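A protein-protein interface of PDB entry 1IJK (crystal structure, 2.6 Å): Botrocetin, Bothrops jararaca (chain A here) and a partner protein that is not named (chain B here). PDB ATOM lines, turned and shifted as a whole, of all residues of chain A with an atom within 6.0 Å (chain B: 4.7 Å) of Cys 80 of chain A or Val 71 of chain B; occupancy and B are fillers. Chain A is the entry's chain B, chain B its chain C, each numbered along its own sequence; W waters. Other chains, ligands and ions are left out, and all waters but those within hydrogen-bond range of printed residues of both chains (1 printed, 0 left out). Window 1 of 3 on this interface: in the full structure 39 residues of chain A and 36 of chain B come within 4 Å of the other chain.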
ATOM      1  N   VAL A  73       2.248  20.534 -13.659  1.00  0.00           N
ATOM      2  CA  VAL A  73       1.395  19.854 -14.620  1.00  0.00           C
ATOM      3  C   VAL A  73       0.257  20.835 -14.907  1.00  0.00           C
ATOM      4  O   VAL A  73      -0.325  21.400 -13.975  1.00  0.00           O
ATOM      5  CB  VAL A  73       0.844  18.534 -14.016  1.00  0.00           C
ATOM      6  CG1 VAL A  73      -0.455  18.112 -14.721  1.00  0.00           C
ATOM      7  CG2 VAL A  73       1.911  17.446 -14.118  1.00  0.00           C
ATOM      8  N   ASN A  75      -2.698  20.138 -16.850  1.00  0.00           N
ATOM      9  CA  ASN A  75      -4.027  19.519 -16.913  1.00  0.00           C
ATOM     10  C   ASN A  75      -4.801  19.682 -15.602  1.00  0.00           C
ATOM     11  O   ASN A  75      -4.222  19.592 -14.522  1.00  0.00           O
ATOM     12  CB  ASN A  75      -3.921  18.018 -17.214  1.00  0.00           C
ATOM     13  CG  ASN A  75      -3.072  17.713 -18.426  1.00  0.00           C
ATOM     14  OD1 ASN A  75      -3.309  16.724 -19.111  1.00  0.00           O
ATOM     15  ND2 ASN A  75      -2.062  18.542 -18.685  1.00  0.00           N
ATOM     16  N   GLU A  77      -7.175  17.655 -14.619  1.00  0.00           N
ATOM     17  CA  GLU A  77      -7.397  16.305 -14.115  1.00  0.00           C
ATOM     18  C   GLU A  77      -6.376  15.856 -13.065  1.00  0.00           C
ATOM     19  O   GLU A  77      -5.305  16.445 -12.942  1.00  0.00           O
ATOM     20  CB  GLU A  77      -7.394  15.328 -15.282  1.00  0.00           C
ATOM     21  CG  GLU A  77      -8.405  15.664 -16.349  1.00  0.00           C
ATOM     22  CD  GLU A  77      -7.990  16.852 -17.192  1.00  0.00           C
ATOM     23  OE1 GLU A  77      -6.993  16.727 -17.943  1.00  0.00           O
ATOM     24  OE2 GLU A  77      -8.659  17.908 -17.104  1.00  0.00           O
ATOM     25  N   LYS A  78      -6.716  14.805 -12.322  1.00  0.00           N
ATOM     26  CA  LYS A  78      -5.831  14.278 -11.286  1.00  0.00           C
ATOM     27  C   LYS A  78      -4.719  13.400 -11.881  1.00  0.00           C
ATOM     28  O   LYS A  78      -3.745  13.069 -11.204  1.00  0.00           O
ATOM     29  CB  LYS A  78      -6.642  13.483 -10.258  1.00  0.00           C
ATOM     30  CG  LYS A  78      -7.921  14.184  -9.840  1.00  0.00           C
ATOM     31  CD  LYS A  78      -8.649  13.468  -8.713  1.00  0.00           C
ATOM     32  CE  LYS A  78     -10.103  13.957  -8.592  1.00  0.00           C
ATOM     33  NZ  LYS A  78     -10.249  15.430  -8.330  1.00  0.00           N
ATOM     34  N   GLN A  79      -4.881  13.020 -13.145  1.00  0.00           N
ATOM     35  CA  GLN A  79      -3.902  12.214 -13.867  1.00  0.00           C
ATOM     36  C   GLN A  79      -4.165  12.497 -15.342  1.00  0.00           C
ATOM     37  O   GLN A  79      -5.310  12.587 -15.765  1.00  0.00           O
ATOM     38  CB  GLN A  79      -4.035  10.714 -13.517  1.00  0.00           C
ATOM     39  CG  GLN A  79      -5.388  10.042 -13.758  1.00  0.00           C
ATOM     40  CD  GLN A  79      -5.638   9.697 -15.218  1.00  0.00           C
ATOM     41  OE1 GLN A  79      -4.761   9.166 -15.903  1.00  0.00           O
ATOM     42  NE2 GLN A  79      -6.844   9.987 -15.696  1.00  0.00           N
ATOM     43  N   CYS A  80      -3.107  12.636 -16.127  1.00  0.00           N
ATOM     44  CA  CYS A  80      -3.269  12.996 -17.523  1.00  0.00           C
ATOM     45  C   CYS A  80      -3.407  11.906 -18.554  1.00  0.00           C
ATOM     46  O   CYS A  80      -3.100  12.130 -19.725  1.00  0.00           O
ATOM     47  CB  CYS A  80      -2.131  13.923 -17.940  1.00  0.00           C
ATOM     48  SG  CYS A  80      -1.651  15.098 -16.640  1.00  0.00           S
ATOM     49  N   SER A  81      -3.866  10.728 -18.155  1.00  0.00           N
ATOM     50  CA  SER A  81      -4.042   9.682 -19.153  1.00  0.00           C
ATOM     51  C   SER A  81      -5.429   9.888 -19.743  1.00  0.00           C
ATOM     52  O   SER A  81      -6.426   9.863 -19.030  1.00  0.00           O
ATOM     53  CB  SER A  81      -3.925   8.289 -18.531  1.00  0.00           C
ATOM     54  OG  SER A  81      -3.569   7.339 -19.518  1.00  0.00           O
ATOM     55  N   SER A  82      -5.473  10.127 -21.047  1.00  0.00           N
ATOM     56  CA  SER A  82      -6.721  10.359 -21.763  1.00  0.00           C
ATOM     57  C   SER A  82      -7.534   9.080 -21.924  1.00  0.00           C
ATOM     58  O   SER A  82      -8.740   9.072 -21.664  1.00  0.00           O
ATOM     59  CB  SER A  82      -6.420  10.952 -23.141  1.00  0.00           C
ATOM     60  OG  SER A  82      -7.405  10.589 -24.093  1.00  0.00           O
ATOM     61  N   LYS A 102       1.756  16.826  -9.229  1.00  0.00           N
ATOM     62  CA  LYS A 102       1.777  17.795 -10.320  1.00  0.00           C
ATOM     63  C   LYS A 102       2.733  18.962 -10.209  1.00  0.00           C
ATOM     64  O   LYS A 102       2.889  19.719 -11.163  1.00  0.00           O
ATOM     65  CB  LYS A 102       0.347  18.304 -10.575  1.00  0.00           C
ATOM     66  CG  LYS A 102      -0.518  17.261 -11.295  1.00  0.00           C
ATOM     67  CD  LYS A 102      -2.003  17.384 -10.991  1.00  0.00           C
ATOM     68  CE  LYS A 102      -2.697  18.324 -11.939  1.00  0.00           C
ATOM     69  NZ  LYS A 102      -4.100  18.536 -11.512  1.00  0.00           N
ATOM     70  N   LEU B  68      -4.252   2.103 -16.836  1.00  0.00           N
ATOM     71  CA  LEU B  68      -3.811   3.493 -16.936  1.00  0.00           C
ATOM     72  C   LEU B  68      -2.296   3.569 -16.752  1.00  0.00           C
ATOM     73  O   LEU B  68      -1.763   3.276 -15.686  1.00  0.00           O
ATOM     74  CB  LEU B  68      -4.546   4.372 -15.920  1.00  0.00           C
ATOM     75  CG  LEU B  68      -6.032   4.590 -16.253  1.00  0.00           C
ATOM     76  CD1 LEU B  68      -6.668   5.548 -15.255  1.00  0.00           C
ATOM     77  CD2 LEU B  68      -6.165   5.133 -17.669  1.00  0.00           C
ATOM     78  N   SER B  69      -1.616   3.983 -17.813  1.00  0.00           N
ATOM     79  CA  SER B  69      -0.161   4.055 -17.855  1.00  0.00           C
ATOM     80  C   SER B  69       0.406   5.456 -18.128  1.00  0.00           C
ATOM     81  O   SER B  69      -0.270   6.303 -18.702  1.00  0.00           O
ATOM     82  CB  SER B  69       0.305   3.063 -18.923  1.00  0.00           C
ATOM     83  OG  SER B  69       1.603   3.339 -19.395  1.00  0.00           O
ATOM     84  N   ASP B  70       1.652   5.676 -17.700  1.00  0.00           N
ATOM     85  CA  ASP B  70       2.387   6.935 -17.874  1.00  0.00           C
ATOM     86  C   ASP B  70       1.531   8.181 -17.660  1.00  0.00           C
ATOM     87  O   ASP B  70       1.549   9.094 -18.476  1.00  0.00           O
ATOM     88  CB  ASP B  70       3.009   6.961 -19.270  1.00  0.00           C
ATOM     89  CG  ASP B  70       4.145   7.958 -19.387  1.00  0.00           C
ATOM     90  OD1 ASP B  70       4.687   8.384 -18.343  1.00  0.00           O
ATOM     91  OD2 ASP B  70       4.516   8.302 -20.530  1.00  0.00           O
ATOM     92  N   VAL B  71       0.818   8.228 -16.538  1.00  0.00           N
ATOM     93  CA  VAL B  71      -0.098   9.322 -16.232  1.00  0.00           C
ATOM     94  C   VAL B  71       0.455  10.722 -16.025  1.00  0.00           C
ATOM     95  O   VAL B  71      -0.330  11.677 -15.917  1.00  0.00           O
ATOM     96  CB  VAL B  71      -0.958   9.003 -14.982  1.00  0.00           C
ATOM     97  CG1 VAL B  71      -1.703   7.698 -15.178  1.00  0.00           C
ATOM     98  CG2 VAL B  71      -0.081   8.965 -13.737  1.00  0.00           C
ATOM     99  N   TRP B  72       1.781  10.861 -15.950  1.00  0.00           N
ATOM    100  CA  TRP B  72       2.376  12.184 -15.737  1.00  0.00           C
ATOM    101  C   TRP B  72       3.063  12.730 -16.966  1.00  0.00           C
ATOM    102  O   TRP B  72       2.993  13.921 -17.241  1.00  0.00           O
ATOM    103  CB  TRP B  72       3.374  12.149 -14.582  1.00  0.00           C
ATOM    104  CG  TRP B  72       2.734  11.835 -13.271  1.00  0.00           C
ATOM    105  CD1 TRP B  72       3.162  10.921 -12.350  1.00  0.00           C
ATOM    106  CD2 TRP B  72       1.524  12.390 -12.755  1.00  0.00           C
ATOM    107  NE1 TRP B  72       2.285  10.866 -11.301  1.00  0.00           N
ATOM    108  CE2 TRP B  72       1.269  11.757 -11.523  1.00  0.00           C
ATOM    109  CE3 TRP B  72       0.627  13.357 -13.218  1.00  0.00           C
ATOM    110  CZ2 TRP B  72       0.148  12.057 -10.744  1.00  0.00           C
ATOM    111  CZ3 TRP B  72      -0.484  13.658 -12.449  1.00  0.00           C
ATOM    112  CH2 TRP B  72      -0.716  13.009 -11.221  1.00  0.00           C
ATOM    113  N   ASN B  73       3.727  11.859 -17.712  1.00  0.00           N
ATOM    114  CA  ASN B  73       4.414  12.308 -18.901  1.00  0.00           C
ATOM    115  C   ASN B  73       3.460  12.577 -20.053  1.00  0.00           C
ATOM    116  O   ASN B  73       3.867  13.072 -21.098  1.00  0.00           O
ATOM    117  CB  ASN B  73       5.507  11.312 -19.263  1.00  0.00           C
ATOM    118  CG  ASN B  73       6.696  11.413 -18.312  1.00  0.00           C
ATOM    119  OD1 ASN B  73       7.358  12.445 -18.239  1.00  0.00           O
ATOM    120  ND2 ASN B  73       6.956  10.355 -17.569  1.00  0.00           N
ATOM    121  N   LYS B  74       2.183  12.267 -19.836  1.00  0.00           N
ATOM    122  CA  LYS B  74       1.125  12.510 -20.817  1.00  0.00           C
ATOM    123  C   LYS B  74       0.442  13.814 -20.429  1.00  0.00           C
ATOM    124  O   LYS B  74      -0.696  14.070 -20.801  1.00  0.00           O
ATOM    125  CB  LYS B  74       0.075  11.401 -20.781  1.00  0.00           C
ATOM    126  CG  LYS B  74       0.535  10.062 -21.291  1.00  0.00           C
ATOM    127  CD  LYS B  74      -0.526   9.029 -20.983  1.00  0.00           C
ATOM    128  CE  LYS B  74      -0.193   7.704 -21.611  1.00  0.00           C
ATOM    129  NZ  LYS B  74      -1.274   6.725 -21.319  1.00  0.00           N
ATOM    130  N   CYS B  75       1.143  14.634 -19.665  1.00  0.00           N
ATOM    131  CA  CYS B  75       0.588  15.890 -19.217  1.00  0.00           C
ATOM    132  C   CYS B  75       1.130  17.049 -20.020  1.00  0.00           C
ATOM    133  O   CYS B  75       2.103  16.916 -20.772  1.00  0.00           O
ATOM    134  CB  CYS B  75       0.928  16.141 -17.744  1.00  0.00           C
ATOM    135  SG  CYS B  75       0.355  14.885 -16.564  1.00  0.00           S
ATOM    136  N   GLU B  97       4.705   6.765 -13.847  1.00  0.00           N
ATOM    137  CA  GLU B  97       3.719   6.192 -12.936  1.00  0.00           C
ATOM    138  C   GLU B  97       2.454   5.606 -13.588  1.00  0.00           C
ATOM    139  O   GLU B  97       2.013   6.018 -14.661  1.00  0.00           O
ATOM    140  CB  GLU B  97       3.367   7.211 -11.837  1.00  0.00           C
ATOM    141  CG  GLU B  97       4.541   7.497 -10.888  1.00  0.00           C
ATOM    142  CD  GLU B  97       4.119   8.208  -9.606  1.00  0.00           C
ATOM    143  OE1 GLU B  97       3.237   9.083  -9.671  1.00  0.00           O
ATOM    144  OE2 GLU B  97       4.670   7.905  -8.526  1.00  0.00           O
ATOM    145  N   VAL B  99      -1.550   3.395 -12.714  1.00  0.00           N
ATOM    146  CA  VAL B  99      -2.654   3.324 -11.759  1.00  0.00           C
ATOM    147  C   VAL B  99      -2.967   1.915 -11.271  1.00  0.00           C
ATOM    148  O   VAL B  99      -3.096   0.985 -12.062  1.00  0.00           O
ATOM    149  CB  VAL B  99      -3.934   3.936 -12.366  1.00  0.00           C
ATOM    150  CG1 VAL B  99      -5.040   3.985 -11.322  1.00  0.00           C
ATOM    151  CG2 VAL B  99      -3.642   5.338 -12.878  1.00  0.00           C
ATOM    152  N   ILE B 110      -1.971   6.118  -7.789  1.00  0.00           N
ATOM    153  CA  ILE B 110      -1.022   6.376  -8.867  1.00  0.00           C
ATOM    154  C   ILE B 110       0.304   6.049  -8.197  1.00  0.00           C
ATOM    155  O   ILE B 110       0.655   6.659  -7.197  1.00  0.00           O
ATOM    156  CB  ILE B 110      -1.012   7.845  -9.297  1.00  0.00           C
ATOM    157  CG1 ILE B 110      -2.409   8.277  -9.731  1.00  0.00           C
ATOM    158  CG2 ILE B 110      -0.058   8.026 -10.459  1.00  0.00           C
ATOM    159  CD1 ILE B 110      -2.568   9.767  -9.917  1.00  0.00           C
HETATM  160  O   HOH W   1      -2.485  16.041 -21.357  1.00  0.00           O
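N of Cys 80 of chain A sits at hydrogen-bond distance from O of Val 71 of chain B (2.9 Å). SG of Cys 80 of chain A forms a disulfide with SG of Cys 75 of chain B (2.0 Å). The side-chain hydroxyl (OG) of Ser 81 of chain A is in hydrogen-bond range of the side-chain amino group (NZ) of Lys 74 of chain B, at 3.0 Å. The backbone carbonyl oxygen (O) of Lys 74 of chain B sits close to the backbone carbonyl oxygen (O) of Cys 80 of chain A (3.3 Å).
N of Val 73 of chain A lies within hydrogen-bond range of O of Lys 102 of chain A, 2.7 Å away. The backbone carbonyl oxygen of Asn 75 of chain A is in hydrogen-bond range of the side-chain amino group of Lys 102 of chain A (3.2 Å). O of Glu 77 of chain A lies within hydrogen-bond range of NZ of Lys 102 of chain A, at 2.8 Å. The backbone carbonyl oxygen of Leu 68 of chain B sits at hydrogen-bond distance from the backbone NH of Val 99 of chain B (3.0 Å). O of Ser 69 of chain B lies within hydrogen-bond range of NZ of Lys 74 of chain B, 2.8 Å away. The backbone NH (N) of Val 71 of chain B sits at hydrogen-bond distance from the backbone carbonyl oxygen (O) of Glu 97 of chain B (3.1 Å).
Among the printed residues, pairs that only touch across the chains: Lys 78 of chain A with Trp 72 of chain B (3.0 Å), Gln 79 of chain A with Val 71 of chain B (3.5 Å), Ser 81 of chain A with Ser 69 of chain B (3.6 Å), Lys 78 of chain A with Ile 110 of chain B (3.7 Å), Asn 75 of chain A with Cys 75 of chain B (3.8 Å), Lys 102 of chain A with Trp 72 of chain B (3.8 Å), Val 73 of chain A with Cys 75 of chain B (3.8 Å), Ser 81 of chain A with Leu 68 of chain B (3.9 Å) and Gln 79 of chain A with Trp 72 of chain B (3.97 Å).
Of the printed residues of chain B, Asn 75 of chain A touches Cys 75. Printed residues of chain B within 4 Å of Cys 80 of chain A: Val 71, Lys 74 and Cys 75. Printed residues of chain B within 4 Å of Ser 81 of chain A: Leu 68, Ser 69 and Lys 74. Of chain A, only Gln 79 and Cys 80 come within 4 Å of Val 71 of chain B. Asn 73 of chain B touches none of the printed residues of chain A. Of the printed residues of chain A, Ile 110 of chain B touches Lys 78. The nearest residue of chain B that does not touch Cys 80 of chain A is Trp 72 of chain B (4.5 Å). The nearest printed residue of chain A that does not touch Ser 69 of chain B is Gln 79 of chain A (6.0 Å).
Of the 9 printed residues of chain A, 7 touch a printed residue of chain B. Printed residues of chain A that touch a printed residue of chain B: Val 73, Asn 75, Lys 78, Gln 79, Cys 80, Ser 81 and Lys 102. Hydrophobic or aromatic side chains of chain A within 4 Å of the printed part of chain B: Val 73. Printed residues of chain B that touch a printed residue of chain A: Leu 68, Ser 69, Val 71, Trp 72, Lys 74, Cys 75 and Ile 110. Hydrophobic or aromatic side chains of chain B that line the printed part of chain A: Leu 68, Val 71, Trp 72 and Ile 110. Among the printed residues, no Asp or Glu carboxylate lies within 4 Å of a Lys or Arg side-chain nitrogen of the other chain.
Water W1 bridges the side-chain amide oxygen (OD1) of Asn 75 of chain A (2.5 Å) and the backbone carbonyl oxygen (O) of Lys 74 of chain B (2.7 Å).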
